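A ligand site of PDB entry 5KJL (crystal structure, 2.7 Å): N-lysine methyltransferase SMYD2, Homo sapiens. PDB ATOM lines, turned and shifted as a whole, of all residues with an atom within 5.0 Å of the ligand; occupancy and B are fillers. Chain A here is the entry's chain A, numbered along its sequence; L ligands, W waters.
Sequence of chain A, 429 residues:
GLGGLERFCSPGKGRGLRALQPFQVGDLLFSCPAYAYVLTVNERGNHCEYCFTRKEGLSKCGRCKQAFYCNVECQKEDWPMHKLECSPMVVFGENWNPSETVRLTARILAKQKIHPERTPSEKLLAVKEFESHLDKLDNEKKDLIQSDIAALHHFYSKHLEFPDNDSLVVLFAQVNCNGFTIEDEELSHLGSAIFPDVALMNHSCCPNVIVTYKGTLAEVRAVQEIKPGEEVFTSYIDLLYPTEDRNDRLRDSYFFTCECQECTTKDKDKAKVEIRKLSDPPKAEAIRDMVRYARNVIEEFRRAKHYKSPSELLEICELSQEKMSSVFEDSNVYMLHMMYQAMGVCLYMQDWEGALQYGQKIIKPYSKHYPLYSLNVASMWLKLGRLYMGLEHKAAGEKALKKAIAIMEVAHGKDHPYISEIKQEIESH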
ATOM      1  N   GLY A  12      16.829  11.971  -9.547  1.00  0.00           N
ATOM      2  CA  GLY A  12      15.377  11.853  -9.650  1.00  0.00           C
ATOM      3  C   GLY A  12      14.646  11.480  -8.374  1.00  0.00           C
ATOM      4  O   GLY A  12      13.481  11.111  -8.424  1.00  0.00           O
ATOM      5  N   LYS A  13      15.327  11.542  -7.236  1.00  0.00           N
ATOM      6  CA  LYS A  13      14.735  11.205  -5.944  1.00  0.00           C
ATOM      7  C   LYS A  13      15.186  12.229  -4.899  1.00  0.00           C
ATOM      8  O   LYS A  13      15.125  11.927  -3.703  1.00  0.00           O
ATOM      9  CB  LYS A  13      15.138   9.771  -5.507  1.00  0.00           C
ATOM     10  CG  LYS A  13      14.861   8.681  -6.553  1.00  0.00           C
ATOM     11  CD  LYS A  13      14.911   7.268  -6.008  1.00  0.00           C
ATOM     12  CE  LYS A  13      14.917   6.270  -7.144  1.00  0.00           C
ATOM     13  NZ  LYS A  13      16.251   6.175  -7.773  1.00  0.00           N
ATOM     14  N   GLY A  14      15.622  13.420  -5.342  1.00  0.00           N
ATOM     15  CA  GLY A  14      16.129  14.510  -4.510  1.00  0.00           C
ATOM     16  C   GLY A  14      17.335  14.088  -3.696  1.00  0.00           C
ATOM     17  O   GLY A  14      18.299  13.556  -4.254  1.00  0.00           O
ATOM     18  N   ARG A  15      17.286  14.288  -2.354  1.00  0.00           N
ATOM     19  CA  ARG A  15      18.361  13.869  -1.445  1.00  0.00           C
ATOM     20  C   ARG A  15      18.106  12.414  -0.960  1.00  0.00           C
ATOM     21  O   ARG A  15      16.950  11.940  -0.968  1.00  0.00           O
ATOM     22  CB  ARG A  15      18.517  14.842  -0.259  1.00  0.00           C
ATOM     23  CG  ARG A  15      19.078  16.204  -0.665  1.00  0.00           C
ATOM     24  CD  ARG A  15      18.686  17.347   0.262  1.00  0.00           C
ATOM     25  NE  ARG A  15      17.252  17.341   0.600  1.00  0.00           N
ATOM     26  CZ  ARG A  15      16.618  18.289   1.274  1.00  0.00           C
ATOM     27  NH1 ARG A  15      15.331  18.175   1.525  1.00  0.00           N
ATOM     28  NH2 ARG A  15      17.272  19.378   1.679  1.00  0.00           N
ATOM     29  N   LEU A 125      19.888  15.269   8.038  1.00  0.00           N
ATOM     30  CA  LEU A 125      18.798  16.115   7.522  1.00  0.00           C
ATOM     31  C   LEU A 125      18.258  16.983   8.661  1.00  0.00           C
ATOM     32  O   LEU A 125      18.000  16.487   9.762  1.00  0.00           O
ATOM     33  CB  LEU A 125      17.657  15.267   6.928  1.00  0.00           C
ATOM     34  CG  LEU A 125      17.049  15.635   5.549  1.00  0.00           C
ATOM     35  CD1 LEU A 125      15.609  15.135   5.438  1.00  0.00           C
ATOM     36  CD2 LEU A 125      17.118  17.101   5.234  1.00  0.00           C
ATOM     37  N   GLU A 129      15.099  21.993   6.404  1.00  0.00           N
ATOM     38  CA  GLU A 129      15.412  21.536   5.047  1.00  0.00           C
ATOM     39  C   GLU A 129      14.379  20.517   4.522  1.00  0.00           C
ATOM     40  O   GLU A 129      14.649  19.892   3.498  1.00  0.00           O
ATOM     41  CB  GLU A 129      16.770  20.815   5.020  1.00  0.00           C
ATOM     42  CG  GLU A 129      18.002  21.556   5.483  1.00  0.00           C
ATOM     43  CD  GLU A 129      19.209  20.647   5.387  1.00  0.00           C
ATOM     44  OE1 GLU A 129      19.853  20.631   4.309  1.00  0.00           O
ATOM     45  OE2 GLU A 129      19.455  19.875   6.341  1.00  0.00           O
ATOM     46  N   GLU A 131      11.414  18.570   2.652  1.00  0.00           N
ATOM     47  CA  GLU A 131      10.674  18.769   1.381  1.00  0.00           C
ATOM     48  C   GLU A 131       9.197  19.000   1.723  1.00  0.00           C
ATOM     49  O   GLU A 131       8.630  18.294   2.565  1.00  0.00           O
ATOM     50  CB  GLU A 131      10.862  17.574   0.415  1.00  0.00           C
ATOM     51  CG  GLU A 131      10.184  17.757  -0.939  1.00  0.00           C
ATOM     52  CD  GLU A 131      10.696  16.879  -2.070  1.00  0.00           C
ATOM     53  OE1 GLU A 131      10.773  17.376  -3.217  1.00  0.00           O
ATOM     54  OE2 GLU A 131      10.993  15.686  -1.820  1.00  0.00           O
ATOM     55  N   HIS A 133       6.604  20.085  -0.986  1.00  0.00           N
ATOM     56  CA  HIS A 133       5.722  19.880  -2.149  1.00  0.00           C
ATOM     57  C   HIS A 133       4.589  20.909  -2.129  1.00  0.00           C
ATOM     58  O   HIS A 133       3.480  20.651  -2.609  1.00  0.00           O
ATOM     59  CB  HIS A 133       5.169  18.444  -2.286  1.00  0.00           C
ATOM     60  CG  HIS A 133       6.187  17.436  -2.693  1.00  0.00           C
ATOM     61  ND1 HIS A 133       6.353  16.274  -1.978  1.00  0.00           N
ATOM     62  CD2 HIS A 133       7.101  17.480  -3.687  1.00  0.00           C
ATOM     63  CE1 HIS A 133       7.345  15.637  -2.566  1.00  0.00           C
ATOM     64  NE2 HIS A 133       7.814  16.314  -3.610  1.00  0.00           N
ATOM     65  N   CYS A 177       4.815  15.191   4.673  1.00  0.00           N
ATOM     66  CA  CYS A 177       5.804  14.576   3.833  1.00  0.00           C
ATOM     67  C   CYS A 177       6.834  13.758   4.596  1.00  0.00           C
ATOM     68  O   CYS A 177       7.294  12.737   4.077  1.00  0.00           O
ATOM     69  CB  CYS A 177       6.475  15.664   3.007  1.00  0.00           C
ATOM     70  SG  CYS A 177       7.489  15.042   1.651  1.00  0.00           S
ATOM     71  N   ASN A 178       7.241  14.211   5.800  1.00  0.00           N
ATOM     72  CA  ASN A 178       8.321  13.612   6.571  1.00  0.00           C
ATOM     73  C   ASN A 178       7.913  13.033   7.940  1.00  0.00           C
ATOM     74  O   ASN A 178       8.730  12.411   8.628  1.00  0.00           O
ATOM     75  CB  ASN A 178       9.451  14.627   6.725  1.00  0.00           C
ATOM     76  CG  ASN A 178       9.900  15.254   5.426  1.00  0.00           C
ATOM     77  OD1 ASN A 178      10.704  14.700   4.679  1.00  0.00           O
ATOM     78  ND2 ASN A 178       9.347  16.411   5.106  1.00  0.00           N
ATOM     79  N   ALA A 199      13.948  10.437   7.889  1.00  0.00           N
ATOM     80  CA  ALA A 199      13.217  11.068   6.788  1.00  0.00           C
ATOM     81  C   ALA A 199      14.075  11.334   5.497  1.00  0.00           C
ATOM     82  O   ALA A 199      13.511  11.664   4.471  1.00  0.00           O
ATOM     83  CB  ALA A 199      12.536  12.334   7.271  1.00  0.00           C
ATOM     84  N   LEU A 200      15.393  11.129   5.539  1.00  0.00           N
ATOM     85  CA  LEU A 200      16.297  11.325   4.396  1.00  0.00           C
ATOM     86  C   LEU A 200      16.196  10.191   3.402  1.00  0.00           C
ATOM     87  O   LEU A 200      16.513  10.372   2.224  1.00  0.00           O
ATOM     88  CB  LEU A 200      17.767  11.452   4.900  1.00  0.00           C
ATOM     89  CG  LEU A 200      18.886  11.702   3.885  1.00  0.00           C
ATOM     90  CD1 LEU A 200      18.590  12.911   2.986  1.00  0.00           C
ATOM     91  CD2 LEU A 200      20.203  11.867   4.562  1.00  0.00           C
ATOM     92  N   MET A 201      15.782   8.996   3.889  1.00  0.00           N
ATOM     93  CA  MET A 201      15.662   7.758   3.108  1.00  0.00           C
ATOM     94  C   MET A 201      14.539   7.829   2.122  1.00  0.00           C
ATOM     95  O   MET A 201      13.417   8.162   2.479  1.00  0.00           O
ATOM     96  CB  MET A 201      15.491   6.520   4.008  1.00  0.00           C
ATOM     97  CG  MET A 201      16.723   6.208   4.826  1.00  0.00           C
ATOM     98  SD  MET A 201      16.563   4.746   5.863  1.00  0.00           S
ATOM     99  CE  MET A 201      15.224   5.205   6.893  1.00  0.00           C
ATOM    100  N   ASN A 202      14.851   7.481   0.875  1.00  0.00           N
ATOM    101  CA  ASN A 202      13.879   7.431  -0.216  1.00  0.00           C
ATOM    102  C   ASN A 202      13.095   6.102  -0.185  1.00  0.00           C
ATOM    103  O   ASN A 202      13.389   5.241   0.666  1.00  0.00           O
ATOM    104  CB  ASN A 202      14.544   7.753  -1.567  1.00  0.00           C
ATOM    105  CG  ASN A 202      14.866   9.215  -1.713  1.00  0.00           C
ATOM    106  OD1 ASN A 202      14.157  10.101  -1.227  1.00  0.00           O
ATOM    107  ND2 ASN A 202      15.990   9.509  -2.347  1.00  0.00           N
ATOM    108  N   HIS A 203      12.037   5.984  -1.032  1.00  0.00           N
ATOM    109  CA  HIS A 203      11.159   4.821  -1.022  1.00  0.00           C
ATOM    110  C   HIS A 203      11.503   3.798  -2.092  1.00  0.00           C
ATOM    111  O   HIS A 203      11.952   4.144  -3.197  1.00  0.00           O
ATOM    112  CB  HIS A 203       9.662   5.261  -1.151  1.00  0.00           C
ATOM    113  CG  HIS A 203       8.700   4.133  -1.442  1.00  0.00           C
ATOM    114  ND1 HIS A 203       8.570   3.573  -2.718  1.00  0.00           N
ATOM    115  CD2 HIS A 203       7.872   3.455  -0.601  1.00  0.00           C
ATOM    116  CE1 HIS A 203       7.674   2.603  -2.595  1.00  0.00           C
ATOM    117  NE2 HIS A 203       7.241   2.489  -1.342  1.00  0.00           N
ATOM    118  N   PHE A 233      16.962   2.373   1.111  1.00  0.00           N
ATOM    119  CA  PHE A 233      15.569   2.606   0.789  1.00  0.00           C
ATOM    120  C   PHE A 233      14.709   1.885   1.759  1.00  0.00           C
ATOM    121  O   PHE A 233      14.946   0.692   1.999  1.00  0.00           O
ATOM    122  CB  PHE A 233      15.250   2.016  -0.605  1.00  0.00           C
ATOM    123  CG  PHE A 233      15.670   2.784  -1.821  1.00  0.00           C
ATOM    124  CD1 PHE A 233      15.080   4.001  -2.135  1.00  0.00           C
ATOM    125  CD2 PHE A 233      16.605   2.262  -2.705  1.00  0.00           C
ATOM    126  CE1 PHE A 233      15.451   4.700  -3.283  1.00  0.00           C
ATOM    127  CE2 PHE A 233      16.978   2.970  -3.846  1.00  0.00           C
ATOM    128  CZ  PHE A 233      16.407   4.190  -4.122  1.00  0.00           C
ATOM    129  N   TYR A 236       7.384   3.406   2.338  1.00  0.00           N
ATOM    130  CA  TYR A 236       6.543   4.464   2.908  1.00  0.00           C
ATOM    131  C   TYR A 236       5.109   3.956   3.078  1.00  0.00           C
ATOM    132  O   TYR A 236       4.336   4.549   3.830  1.00  0.00           O
ATOM    133  CB  TYR A 236       6.498   5.663   1.926  1.00  0.00           C
ATOM    134  CG  TYR A 236       7.746   6.513   1.719  1.00  0.00           C
ATOM    135  CD1 TYR A 236       8.968   6.175   2.331  1.00  0.00           C
ATOM    136  CD2 TYR A 236       7.716   7.675   0.939  1.00  0.00           C
ATOM    137  CE1 TYR A 236      10.111   6.957   2.148  1.00  0.00           C
ATOM    138  CE2 TYR A 236       8.855   8.463   0.750  1.00  0.00           C
ATOM    139  CZ  TYR A 236      10.056   8.094   1.358  1.00  0.00           C
ATOM    140  OH  TYR A 236      11.178   8.853   1.196  1.00  0.00           O
ATOM    141  N   TYR A 254       2.716  11.591  -1.158  1.00  0.00           N
ATOM    142  CA  TYR A 254       4.120  11.940  -1.286  1.00  0.00           C
ATOM    143  C   TYR A 254       4.501  12.537  -2.636  1.00  0.00           C
ATOM    144  O   TYR A 254       5.684  12.811  -2.863  1.00  0.00           O
ATOM    145  CB  TYR A 254       5.008  10.742  -0.930  1.00  0.00           C
ATOM    146  CG  TYR A 254       4.786  10.228   0.486  1.00  0.00           C
ATOM    147  CD1 TYR A 254       5.377  10.863   1.578  1.00  0.00           C
ATOM    148  CD2 TYR A 254       4.009   9.096   0.728  1.00  0.00           C
ATOM    149  CE1 TYR A 254       5.169  10.390   2.874  1.00  0.00           C
ATOM    150  CE2 TYR A 254       3.785   8.635   2.015  1.00  0.00           C
ATOM    151  CZ  TYR A 254       4.355   9.289   3.092  1.00  0.00           C
ATOM    152  OH  TYR A 254       4.131   8.821   4.356  1.00  0.00           O
ATOM    153  N   PHE A 255       3.497  12.816  -3.499  1.00  0.00           N
ATOM    154  CA  PHE A 255       3.644  13.510  -4.782  1.00  0.00           C
ATOM    155  C   PHE A 255       4.787  13.003  -5.697  1.00  0.00           C
ATOM    156  O   PHE A 255       5.486  13.807  -6.319  1.00  0.00           O
ATOM    157  CB  PHE A 255       3.789  15.039  -4.524  1.00  0.00           C
ATOM    158  CG  PHE A 255       2.706  15.580  -3.640  1.00  0.00           C
ATOM    159  CD1 PHE A 255       1.506  16.043  -4.184  1.00  0.00           C
ATOM    160  CD2 PHE A 255       2.853  15.603  -2.255  1.00  0.00           C
ATOM    161  CE1 PHE A 255       0.478  16.510  -3.362  1.00  0.00           C
ATOM    162  CE2 PHE A 255       1.811  16.040  -1.423  1.00  0.00           C
ATOM    163  CZ  PHE A 255       0.636  16.485  -1.986  1.00  0.00           C
ATOM    164  N   PHE A 256       4.934  11.680  -5.798  1.00  0.00           N
ATOM    165  CA  PHE A 256       5.936  11.053  -6.659  1.00  0.00           C
ATOM    166  C   PHE A 256       5.409   9.733  -7.171  1.00  0.00           C
ATOM    167  O   PHE A 256       4.502   9.163  -6.560  1.00  0.00           O
ATOM    168  CB  PHE A 256       7.293  10.852  -5.927  1.00  0.00           C
ATOM    169  CG  PHE A 256       7.429   9.648  -4.989  1.00  0.00           C
ATOM    170  CD1 PHE A 256       7.910   8.432  -5.458  1.00  0.00           C
ATOM    171  CD2 PHE A 256       7.181   9.778  -3.632  1.00  0.00           C
ATOM    172  CE1 PHE A 256       8.088   7.352  -4.590  1.00  0.00           C
ATOM    173  CE2 PHE A 256       7.348   8.689  -2.766  1.00  0.00           C
ATOM    174  CZ  PHE A 256       7.773   7.481  -3.255  1.00  0.00           C
ATOM    175  N   THR A 257       6.027   9.223  -8.240  1.00  0.00           N
ATOM    176  CA  THR A 257       5.750   7.908  -8.789  1.00  0.00           C
ATOM    177  C   THR A 257       7.007   7.031  -8.621  1.00  0.00           C
ATOM    178  O   THR A 257       8.130   7.445  -8.963  1.00  0.00           O
ATOM    179  CB  THR A 257       5.303   8.015 -10.235  1.00  0.00           C
ATOM    180  OG1 THR A 257       4.161   8.885 -10.309  1.00  0.00           O
ATOM    181  CG2 THR A 257       5.018   6.647 -10.878  1.00  0.00           C
ATOM    182  N   CYS A 258       6.813   5.833  -8.051  1.00  0.00           N
ATOM    183  CA  CYS A 258       7.906   4.904  -7.839  1.00  0.00           C
ATOM    184  C   CYS A 258       8.269   4.198  -9.123  1.00  0.00           C
ATOM    185  O   CYS A 258       7.388   3.830  -9.912  1.00  0.00           O
ATOM    186  CB  CYS A 258       7.572   3.915  -6.743  1.00  0.00           C
ATOM    187  SG  CYS A 258       8.972   2.890  -6.223  1.00  0.00           S
HETATM  188  N1  LIG L   1      14.279  12.885  -1.105  1.00  0.00           N
HETATM  189  C1  LIG L   1      13.810  13.606   0.104  1.00  0.00           C
HETATM  190  C2  LIG L   1      14.542  14.977   0.316  1.00  0.00           C
HETATM  191  O1  LIG L   1      15.414  15.296  -0.528  1.00  0.00           O
HETATM  192  O2  LIG L   1      14.196  15.678   1.293  1.00  0.00           O
HETATM  193  C3  LIG L   1      13.909  12.703   1.368  1.00  0.00           C
HETATM  194  C4  LIG L   1      12.725  11.752   1.480  1.00  0.00           C
HETATM  195  S1  LIG L   1      11.254  12.656   2.037  1.00  0.00           S
HETATM  196  C5  LIG L   1      10.644  11.743   3.405  1.00  0.00           C
HETATM  197  C6  LIG L   1      10.004  12.032   0.793  1.00  0.00           C
HETATM  198  C7  LIG L   1      10.040  12.677  -0.565  1.00  0.00           C
HETATM  199  O3  LIG L   1      11.215  12.242  -1.288  1.00  0.00           O
HETATM  200  C8  LIG L   1       8.879  12.304  -1.469  1.00  0.00           C
HETATM  201  O4  LIG L   1       7.692  13.056  -1.205  1.00  0.00           O
HETATM  202  C9  LIG L   1       9.467  12.468  -2.872  1.00  0.00           C
HETATM  203  O5  LIG L   1       9.532  13.810  -3.310  1.00  0.00           O
HETATM  204  C10 LIG L   1      10.903  11.981  -2.647  1.00  0.00           C
HETATM  205  N2  LIG L   1      11.084  10.551  -2.906  1.00  0.00           N
HETATM  206  C11 LIG L   1      11.249   9.542  -2.005  1.00  0.00           C
HETATM  207  N3  LIG L   1      11.404   8.360  -2.538  1.00  0.00           N
HETATM  208  C12 LIG L   1      11.323   8.600  -3.896  1.00  0.00           C
HETATM  209  C13 LIG L   1      11.394   7.752  -5.028  1.00  0.00           C
HETATM  210  N4  LIG L   1      11.677   6.447  -4.944  1.00  0.00           N
HETATM  211  N5  LIG L   1      11.227   8.307  -6.249  1.00  0.00           N
HETATM  212  C14 LIG L   1      11.022   9.627  -6.333  1.00  0.00           C
HETATM  213  N6  LIG L   1      10.942  10.528  -5.343  1.00  0.00           N
HETATM  214  C15 LIG L   1      11.109   9.945  -4.151  1.00  0.00           C
HETATM  215  O   HOH W   1      12.724  15.835   3.531  1.00  0.00           O
HETATM  216  O   HOH W   2      12.285   3.832  -6.271  1.00  0.00           O
HETATM  217  O   HOH W   3      13.043  14.577  -3.284  1.00  0.00           O
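The side-chain sulfur (SG) of Cys 177 sits at hydrogen-bond distance from an oxygen (O4) of the ligand, at 3.5 Å.
O of Arg 15 lies within hydrogen-bond range of N1 of the ligand (2.8 Å).
O5 of the ligand lies close to NE2 of His 133, at 3.1 Å.
The backbone NH (N) of Arg 15 lies within hydrogen-bond range of an oxygen (O1) of the ligand, 2.8 Å away.
An oxygen (O4) of the ligand sits at hydrogen-bond distance from the backbone carbonyl oxygen (O) of Tyr 254 (2.6 Å).
The side-chain amide oxygen (OD1) of Asn 202 sits at hydrogen-bond distance from a nitrogen (N1) of the ligand (2.8 Å).
A nitrogen (N3) of the ligand is in hydrogen-bond range of the backbone NH (N) of His 203 (2.9 Å).
NH1 of Arg 15 is in salt-bridge range of O2 of the ligand, 2.8 Å away.
The backbone carbonyl oxygen (O) of His 203 lies within hydrogen-bond range of a nitrogen (N4) of the ligand, 2.9 Å away.
The backbone carbonyl oxygen of Lys 13 lies within hydrogen-bond range of a nitrogen (N1) of the ligand (2.9 Å).
An oxygen (O5) of the ligand is in hydrogen-bond range of the side-chain carboxylate (OE2) of Glu 131 (2.8 Å).
The side-chain amide nitrogen (ND2) of Asn 202 is in hydrogen-bond range of the backbone carbonyl oxygen (O) of Lys 13, 2.9 Å away.
NE2 of His 133 sits at hydrogen-bond distance from OE1 of Glu 131.
The side-chain hydroxyl of Tyr 236 lies within hydrogen-bond range of the backbone carbonyl oxygen of Met 201 (2.7 Å).
The guanidinium group (NH2) of Arg 15 is in salt-bridge range of the side-chain carboxylate (OE1) of Glu 129.
The backbone carbonyl oxygen (O) of Arg 15 sits at hydrogen-bond distance from the side-chain amide nitrogen (ND2) of Asn 202 (3.0 Å).
O of Glu 131 sits at hydrogen-bond distance from ND2 of Asn 178.
The side-chain sulfur of Cys 258 lies close to a ring nitrogen (ND1) of His 203, at 3.6 Å.
The backbone carbonyl oxygen of Glu 131 lies close to the side-chain sulfur of Cys 177 (3.6 Å).
S1 of the ligand lies close to OD1 of Asn 178 (3.4 Å).
O of Ala 199 sits close to S1 of the ligand.
Gly 12 touches the ligand (O to C14, 3.6 Å).
C of Gly 14 touches O1 of the ligand, at 3.9 Å.
Leu 200 touches the ligand.
Met 201 touches the ligand.
OH of Tyr 236 touches C11 of the ligand, 3.3 Å away.
CE1 of Phe 256 touches C13 of the ligand, 3.4 Å away.
Hydrophobic or aromatic side chains that line the ligand: His 133, His 203, Tyr 236, Tyr 254 and Phe 256.
Of the 22 residues printed, 16 come within 4 Å of the ligand.
Water W1 lies within hydrogen-bond range of the side-chain amide oxygen of Asn 178 (2.6 Å), an oxygen (O2) of the ligand (2.7 Å) and the backbone NH of Glu 131 (3.2 Å).
Water W2 lies within hydrogen-bond range of N4 of the ligand (3.0 Å) and O of His 203 (3.1 Å).
Water W3 lies within hydrogen-bond range of the side-chain carboxylate (OE2) of Glu 131 (2.8 Å), a nitrogen (N1) of the ligand (3.0 Å), the backbone carbonyl oxygen (O) of Lys 13 (3.4 Å) and the backbone NH (N) of Gly 14 (3.5 Å).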
